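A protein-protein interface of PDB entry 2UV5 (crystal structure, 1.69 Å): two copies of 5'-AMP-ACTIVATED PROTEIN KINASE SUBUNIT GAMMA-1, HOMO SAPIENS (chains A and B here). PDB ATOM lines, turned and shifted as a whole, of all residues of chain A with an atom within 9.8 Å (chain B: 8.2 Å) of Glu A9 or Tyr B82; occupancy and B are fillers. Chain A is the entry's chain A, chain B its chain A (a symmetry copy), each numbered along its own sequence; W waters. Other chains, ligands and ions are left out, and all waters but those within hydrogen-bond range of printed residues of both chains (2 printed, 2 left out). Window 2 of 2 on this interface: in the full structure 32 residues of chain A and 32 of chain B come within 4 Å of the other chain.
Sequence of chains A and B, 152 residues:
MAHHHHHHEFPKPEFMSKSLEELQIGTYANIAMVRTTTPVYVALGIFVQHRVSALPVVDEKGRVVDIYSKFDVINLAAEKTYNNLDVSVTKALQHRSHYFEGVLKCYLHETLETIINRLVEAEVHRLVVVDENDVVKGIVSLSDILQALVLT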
ATOM      1  N   HIS A   8      16.081 -25.777 -14.983  1.00  0.00           N
ATOM      2  CA  HIS A   8      17.179 -26.315 -14.117  1.00  0.00           C
ATOM      3  C   HIS A   8      17.999 -27.309 -14.936  1.00  0.00           C
ATOM      4  O   HIS A   8      18.673 -28.193 -14.421  1.00  0.00           O
ATOM      5  CB  HIS A   8      16.597 -26.989 -12.884  1.00  0.00           C
ATOM      6  CG  HIS A   8      15.818 -28.227 -13.187  1.00  0.00           C
ATOM      7  ND1 HIS A   8      15.362 -28.525 -14.455  1.00  0.00           N
ATOM      8  CD2 HIS A   8      15.400 -29.237 -12.384  1.00  0.00           C
ATOM      9  CE1 HIS A   8      14.702 -29.670 -14.416  1.00  0.00           C
ATOM     10  NE2 HIS A   8      14.704 -30.116 -13.171  1.00  0.00           N
ATOM     11  N   GLU A   9      18.510 -26.205 -16.171  1.00  0.00           N
ATOM     12  CA  GLU A   9      19.593 -26.830 -16.911  1.00  0.00           C
ATOM     13  C   GLU A   9      20.826 -27.011 -16.052  1.00  0.00           C
ATOM     14  O   GLU A   9      21.156 -26.151 -15.219  1.00  0.00           O
ATOM     15  CB  GLU A   9      19.935 -25.972 -18.124  1.00  0.00           C
ATOM     16  CG  GLU A   9      20.924 -26.620 -19.054  1.00  0.00           C
ATOM     17  CD  GLU A   9      21.264 -25.749 -20.242  1.00  0.00           C
ATOM     18  OE1 GLU A   9      22.174 -26.133 -20.983  1.00  0.00           O
ATOM     19  OE2 GLU A   9      20.625 -24.689 -20.441  1.00  0.00           O
ATOM     20  N   PHE A  10      21.494 -28.143 -16.247  1.00  0.00           N
ATOM     21  CA  PHE A  10      22.787 -28.390 -15.646  1.00  0.00           C
ATOM     22  C   PHE A  10      23.870 -28.485 -16.703  1.00  0.00           C
ATOM     23  O   PHE A  10      23.769 -29.260 -17.630  1.00  0.00           O
ATOM     24  CB  PHE A  10      22.821 -29.650 -14.811  1.00  0.00           C
ATOM     25  CG  PHE A  10      24.164 -29.885 -14.172  1.00  0.00           C
ATOM     26  CD1 PHE A  10      24.531 -29.196 -13.002  1.00  0.00           C
ATOM     27  CD2 PHE A  10      25.075 -30.749 -14.752  1.00  0.00           C
ATOM     28  CE1 PHE A  10      25.780 -29.391 -12.426  1.00  0.00           C
ATOM     29  CE2 PHE A  10      26.350 -30.953 -14.177  1.00  0.00           C
ATOM     30  CZ  PHE A  10      26.685 -30.286 -13.012  1.00  0.00           C
ATOM     31  N   PRO A  11      24.907 -27.665 -16.579  1.00  0.00           N
ATOM     32  CA  PRO A  11      25.126 -26.624 -15.595  1.00  0.00           C
ATOM     33  C   PRO A  11      24.355 -25.359 -16.017  1.00  0.00           C
ATOM     34  O   PRO A  11      23.965 -25.249 -17.184  1.00  0.00           O
ATOM     35  CB  PRO A  11      26.637 -26.431 -15.662  1.00  0.00           C
ATOM     36  CG  PRO A  11      26.961 -26.712 -17.088  1.00  0.00           C
ATOM     37  CD  PRO A  11      26.005 -27.739 -17.556  1.00  0.00           C
ATOM     38  N   LYS A  12      24.102 -24.428 -15.095  1.00  0.00           N
ATOM     39  CA  LYS A  12      23.342 -23.228 -15.461  1.00  0.00           C
ATOM     40  C   LYS A  12      24.170 -22.360 -16.398  1.00  0.00           C
ATOM     41  O   LYS A  12      25.317 -22.069 -16.090  1.00  0.00           O
ATOM     42  CB  LYS A  12      22.952 -22.422 -14.227  1.00  0.00           C
ATOM     43  CG  LYS A  12      21.993 -23.143 -13.300  1.00  0.00           C
ATOM     44  CD  LYS A  12      21.270 -22.165 -12.349  1.00  0.00           C
ATOM     45  CE  LYS A  12      22.017 -21.979 -11.034  1.00  0.00           C
ATOM     46  NZ  LYS A  12      21.321 -20.970 -10.178  1.00  0.00           N
ATOM     47  N   PRO A  13      23.594 -21.942 -17.539  1.00  0.00           N
ATOM     48  CA  PRO A  13      24.369 -21.124 -18.486  1.00  0.00           C
ATOM     49  C   PRO A  13      24.955 -19.843 -17.893  1.00  0.00           C
ATOM     50  O   PRO A  13      26.054 -19.454 -18.268  1.00  0.00           O
ATOM     51  CB  PRO A  13      23.341 -20.742 -19.562  1.00  0.00           C
ATOM     52  CG  PRO A  13      22.321 -21.818 -19.491  1.00  0.00           C
ATOM     53  CD  PRO A  13      22.247 -22.244 -18.059  1.00  0.00           C
ATOM     54  N   GLU A  14      24.199 -19.184 -17.026  1.00  0.00           N
ATOM     55  CA  GLU A  14      24.630 -17.915 -16.431  1.00  0.00           C
ATOM     56  C   GLU A  14      25.857 -18.063 -15.537  1.00  0.00           C
ATOM     57  O   GLU A  14      26.552 -17.085 -15.275  1.00  0.00           O
ATOM     58  CB  GLU A  14      23.494 -17.245 -15.647  1.00  0.00           C
ATOM     59  CG  GLU A  14      22.881 -18.097 -14.542  1.00  0.00           C
ATOM     60  CD  GLU A  14      21.639 -18.876 -14.975  1.00  0.00           C
ATOM     61  OE1 GLU A  14      20.739 -19.045 -14.119  1.00  0.00           O
ATOM     62  OE2 GLU A  14      21.567 -19.328 -16.145  1.00  0.00           O
ATOM     63  N   PHE A  15      26.127 -19.274 -15.067  1.00  0.00           N
ATOM     64  CA  PHE A  15      27.357 -19.518 -14.314  1.00  0.00           C
ATOM     65  C   PHE A  15      28.495 -20.052 -15.207  1.00  0.00           C
ATOM     66  O   PHE A  15      29.659 -19.764 -14.953  1.00  0.00           O
ATOM     67  CB  PHE A  15      27.037 -20.357 -13.082  1.00  0.00           C
ATOM     68  CG  PHE A  15      26.144 -19.629 -12.079  1.00  0.00           C
ATOM     69  CD1 PHE A  15      26.688 -18.738 -11.150  1.00  0.00           C
ATOM     70  CD2 PHE A  15      24.765 -19.818 -12.084  1.00  0.00           C
ATOM     71  CE1 PHE A  15      25.883 -18.068 -10.244  1.00  0.00           C
ATOM     72  CE2 PHE A  15      23.949 -19.147 -11.175  1.00  0.00           C
ATOM     73  CZ  PHE A  15      24.512 -18.272 -10.253  1.00  0.00           C
ATOM     74  N   MET A  16      28.167 -20.766 -16.290  1.00  0.00           N
ATOM     75  CA  MET A  16      29.166 -21.151 -17.305  1.00  0.00           C
ATOM     76  C   MET A  16      29.861 -19.967 -17.974  1.00  0.00           C
ATOM     77  O   MET A  16      31.049 -20.054 -18.303  1.00  0.00           O
ATOM     78  CB  MET A  16      28.554 -22.051 -18.370  1.00  0.00           C
ATOM     79  CG  MET A  16      28.181 -23.417 -17.830  1.00  0.00           C
ATOM     80  SD  MET A  16      29.619 -24.408 -17.302  1.00  0.00           S
ATOM     81  CE  MET A  16      29.912 -25.293 -18.841  1.00  0.00           C
ATOM     82  N   GLU A 113      33.022 -22.290 -18.475  1.00  0.00           N
ATOM     83  CA  GLU A 113      32.874 -23.138 -19.660  1.00  0.00           C
ATOM     84  C   GLU A 113      34.234 -23.471 -20.271  1.00  0.00           C
ATOM     85  O   GLU A 113      34.497 -24.609 -20.627  1.00  0.00           O
ATOM     86  CB  GLU A 113      31.989 -22.438 -20.703  1.00  0.00           C
ATOM     87  CG  GLU A 113      31.744 -23.262 -21.942  1.00  0.00           C
ATOM     88  CD  GLU A 113      31.099 -22.439 -23.014  1.00  0.00           C
ATOM     89  OE1 GLU A 113      29.887 -22.162 -22.902  1.00  0.00           O
ATOM     90  OE2 GLU A 113      31.820 -22.038 -23.952  1.00  0.00           O
ATOM     91  N   LEU A 149      29.160 -25.065  -8.531  1.00  0.00           N
ATOM     92  CA  LEU A 149      28.016 -25.596  -9.294  1.00  0.00           C
ATOM     93  C   LEU A 149      26.754 -25.819  -8.470  1.00  0.00           C
ATOM     94  O   LEU A 149      25.674 -25.949  -9.046  1.00  0.00           O
ATOM     95  CB  LEU A 149      28.400 -26.898 -10.015  1.00  0.00           C
ATOM     96  CG  LEU A 149      29.173 -26.751 -11.325  1.00  0.00           C
ATOM     97  CD1 LEU A 149      29.694 -28.109 -11.828  1.00  0.00           C
ATOM     98  CD2 LEU A 149      28.313 -26.067 -12.394  1.00  0.00           C
ATOM     99  N   LEU B  76      29.694 -34.637 -17.398  1.00  0.00           N
ATOM    100  CA  LEU B  76      28.283 -34.319 -17.606  1.00  0.00           C
ATOM    101  C   LEU B  76      28.118 -32.830 -17.874  1.00  0.00           C
ATOM    102  O   LEU B  76      27.455 -32.440 -18.850  1.00  0.00           O
ATOM    103  CB  LEU B  76      27.437 -34.698 -16.391  1.00  0.00           C
ATOM    104  CG  LEU B  76      25.941 -34.421 -16.503  1.00  0.00           C
ATOM    105  CD1 LEU B  76      25.328 -35.320 -17.624  1.00  0.00           C
ATOM    106  CD2 LEU B  76      25.246 -34.616 -15.132  1.00  0.00           C
ATOM    107  N   ALA B  77      28.730 -32.006 -17.017  1.00  0.00           N
ATOM    108  CA  ALA B  77      28.667 -30.542 -17.190  1.00  0.00           C
ATOM    109  C   ALA B  77      29.136 -30.057 -18.578  1.00  0.00           C
ATOM    110  O   ALA B  77      28.581 -29.085 -19.127  1.00  0.00           O
ATOM    111  CB  ALA B  77      29.462 -29.832 -16.079  1.00  0.00           C
ATOM    112  N   GLU B  79      28.940 -31.707 -21.495  1.00  0.00           N
ATOM    113  CA  GLU B  79      28.146 -32.240 -22.629  1.00  0.00           C
ATOM    114  C   GLU B  79      27.401 -31.104 -23.306  1.00  0.00           C
ATOM    115  O   GLU B  79      26.786 -30.281 -22.637  1.00  0.00           O
ATOM    116  CB  GLU B  79      27.159 -33.322 -22.163  1.00  0.00           C
ATOM    117  CG  GLU B  79      27.822 -34.608 -21.736  1.00  0.00           C
ATOM    118  CD  GLU B  79      26.854 -35.677 -21.201  1.00  0.00           C
ATOM    119  OE1 GLU B  79      25.642 -35.627 -21.490  1.00  0.00           O
ATOM    120  OE2 GLU B  79      27.307 -36.586 -20.470  1.00  0.00           O
ATOM    121  N   LYS B  80      27.485 -31.047 -24.632  1.00  0.00           N
ATOM    122  CA  LYS B  80      26.882 -29.942 -25.391  1.00  0.00           C
ATOM    123  C   LYS B  80      25.371 -30.056 -25.473  1.00  0.00           C
ATOM    124  O   LYS B  80      24.667 -29.049 -25.691  1.00  0.00           O
ATOM    125  CB  LYS B  80      27.536 -29.860 -26.770  1.00  0.00           C
ATOM    126  CG  LYS B  80      28.993 -29.407 -26.650  1.00  0.00           C
ATOM    127  CD  LYS B  80      29.817 -29.635 -27.908  1.00  0.00           C
ATOM    128  CE  LYS B  80      31.285 -29.241 -27.672  1.00  0.00           C
ATOM    129  NZ  LYS B  80      31.448 -27.933 -26.937  1.00  0.00           N
ATOM    130  N   THR B  81      24.866 -31.273 -25.290  1.00  0.00           N
ATOM    131  CA  THR B  81      23.427 -31.521 -25.277  1.00  0.00           C
ATOM    132  C   THR B  81      22.812 -31.022 -23.967  1.00  0.00           C
ATOM    133  O   THR B  81      23.529 -30.818 -22.986  1.00  0.00           O
ATOM    134  CB  THR B  81      23.117 -33.019 -25.473  1.00  0.00           C
ATOM    135  OG1 THR B  81      23.982 -33.801 -24.635  1.00  0.00           O
ATOM    136  CG2 THR B  81      23.322 -33.413 -26.942  1.00  0.00           C
ATOM    137  N   TYR B  82      21.492 -30.831 -23.960  1.00  0.00           N
ATOM    138  CA  TYR B  82      20.778 -30.330 -22.780  1.00  0.00           C
ATOM    139  C   TYR B  82      20.608 -31.446 -21.722  1.00  0.00           C
ATOM    140  O   TYR B  82      20.029 -32.521 -21.985  1.00  0.00           O
ATOM    141  CB  TYR B  82      19.419 -29.744 -23.164  1.00  0.00           C
ATOM    142  CG  TYR B  82      18.680 -29.082 -22.030  1.00  0.00           C
ATOM    143  CD1 TYR B  82      18.696 -27.696 -21.866  1.00  0.00           C
ATOM    144  CD2 TYR B  82      17.969 -29.842 -21.104  1.00  0.00           C
ATOM    145  CE1 TYR B  82      18.001 -27.083 -20.808  1.00  0.00           C
ATOM    146  CE2 TYR B  82      17.274 -29.250 -20.058  1.00  0.00           C
ATOM    147  CZ  TYR B  82      17.291 -27.881 -19.910  1.00  0.00           C
ATOM    148  OH  TYR B  82      16.587 -27.335 -18.856  1.00  0.00           O
ATOM    149  N   ASN B  83      21.129 -31.173 -20.534  1.00  0.00           N
ATOM    150  CA  ASN B  83      20.905 -32.010 -19.358  1.00  0.00           C
ATOM    151  C   ASN B  83      20.403 -31.190 -18.188  1.00  0.00           C
ATOM    152  O   ASN B  83      20.566 -29.968 -18.154  1.00  0.00           O
ATOM    153  CB  ASN B  83      22.211 -32.687 -18.919  1.00  0.00           C
ATOM    154  CG  ASN B  83      22.779 -33.601 -19.982  1.00  0.00           C
ATOM    155  OD1 ASN B  83      22.144 -34.582 -20.374  1.00  0.00           O
ATOM    156  ND2 ASN B  83      23.971 -33.268 -20.474  1.00  0.00           N
ATOM    157  N   ASN B  84      19.771 -31.883 -17.248  1.00  0.00           N
ATOM    158  CA  ASN B  84      19.531 -31.370 -15.886  1.00  0.00           C
ATOM    159  C   ASN B  84      20.065 -32.379 -14.870  1.00  0.00           C
ATOM    160  O   ASN B  84      20.615 -33.407 -15.243  1.00  0.00           O
ATOM    161  CB  ASN B  84      18.053 -31.051 -15.635  1.00  0.00           C
ATOM    162  CG  ASN B  84      17.135 -32.232 -15.908  1.00  0.00           C
ATOM    163  OD1 ASN B  84      17.398 -33.340 -15.482  1.00  0.00           O
ATOM    164  ND2 ASN B  84      16.039 -31.985 -16.608  1.00  0.00           N
ATOM    165  N   LEU B  85      19.899 -32.104 -13.592  1.00  0.00           N
ATOM    166  CA  LEU B  85      20.499 -32.977 -12.590  1.00  0.00           C
ATOM    167  C   LEU B  85      19.641 -34.185 -12.248  1.00  0.00           C
ATOM    168  O   LEU B  85      20.050 -35.041 -11.455  1.00  0.00           O
ATOM    169  CB  LEU B  85      20.808 -32.191 -11.326  1.00  0.00           C
ATOM    170  CG  LEU B  85      22.056 -31.329 -11.354  1.00  0.00           C
ATOM    171  CD1 LEU B  85      22.074 -30.478 -10.096  1.00  0.00           C
ATOM    172  CD2 LEU B  85      23.304 -32.189 -11.443  1.00  0.00           C
ATOM    173  N   VAL B  87      18.970 -36.832 -13.864  1.00  0.00           N
ATOM    174  CA  VAL B  87      19.321 -37.983 -14.700  1.00  0.00           C
ATOM    175  C   VAL B  87      20.084 -38.939 -13.773  1.00  0.00           C
ATOM    176  O   VAL B  87      20.753 -38.465 -12.850  1.00  0.00           O
ATOM    177  CB  VAL B  87      20.166 -37.536 -15.921  1.00  0.00           C
ATOM    178  CG1 VAL B  87      21.488 -36.934 -15.487  1.00  0.00           C
ATOM    179  CG2 VAL B  87      20.367 -38.683 -16.894  1.00  0.00           C
ATOM    180  N   LYS B  91      24.063 -42.539 -16.470  1.00  0.00           N
ATOM    181  CA  LYS B  91      24.367 -41.898 -17.736  1.00  0.00           C
ATOM    182  C   LYS B  91      25.876 -41.746 -17.965  1.00  0.00           C
ATOM    183  O   LYS B  91      26.333 -41.689 -19.109  1.00  0.00           O
ATOM    184  CB  LYS B  91      23.623 -40.575 -17.925  1.00  0.00           C
ATOM    185  CG  LYS B  91      23.440 -40.287 -19.432  1.00  0.00           C
ATOM    186  CD  LYS B  91      22.482 -39.132 -19.762  1.00  0.00           C
ATOM    187  CE  LYS B  91      23.205 -37.857 -20.079  1.00  0.00           C
ATOM    188  NZ  LYS B  91      24.015 -37.876 -21.310  1.00  0.00           N
HETATM  189  O   HOH W   1      15.384 -29.013 -17.489  1.00  0.00           O
HETATM  190  O   HOH W   2      25.306 -30.705 -19.436  1.00  0.00           O
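No position is printed for both chains.
Glu A9 touches just these residues of chain B: Tyr B82 and Asn B83. Of the printed residues of chain B, Phe A10 touches Leu B76, Ala B77, Asn B83, Asn B84 and Leu B85. Printed residues of chain B within 4 Å of Pro A11: Ala B77. Phe A15 touches none of the printed residues of chain B. No residue of chain A comes within 4 Å of Thr B81. Of chain A, only Glu A9 comes within 4 Å of Tyr B82. Asn B83 touches just these residues of chain A: Glu A9 (3.5 Å) and Phe A10 (2.8 Å). Lys B91 touches none of the printed residues of chain A. The nearest printed residue of chain A that does not touch Leu B76 is Pro A11 (5.1 Å).
ND2 of Asn B83 is in hydrogen-bond range of OE1 of Glu B79, 3.1 Å away.
Of the 11 printed residues of chain B, 6 touch a printed residue of chain A. Along chain B the printed residues that touch a printed residue of chain A span positions 76 to 85. Hydrophobic or aromatic side chains of chain A that line the printed part of chain B: His A8, Phe A10 and Pro A11. Among the printed residues, 9 pairs touch across the chains.
Water W1 lies within hydrogen-bond range of OH of Tyr B82, ND1 of His A8 and ND2 of Asn B84. Water W2 lies within hydrogen-bond range of the backbone carbonyl oxygen (O) of Phe A10 (2.8 Å), the backbone carbonyl oxygen (O) of Leu B76 (2.8 Å) and the side-chain amide nitrogen (ND2) of Asn B83 (3.1 Å).
Among the printed residues, pairs that only touch across the chains: His A8 with Asn B84 (3.2 Å), Glu A9 with Asn B83 (3.5 Å), Phe A10 with Leu B76 (3.9 Å), Phe A10 with Ala B77 (3.8 Å), Phe A10 with Asn B84 (3.8 Å), Phe A10 with Leu B85 (3.6 Å) and Pro A11 with Ala B77 (3.3 Å).
The side-chain hydroxyl of Tyr B82 lies within hydrogen-bond range of the backbone NH of Glu A9 (3.5 Å). O of Asn B83 is in hydrogen-bond range of N of Phe A10 (2.8 Å).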
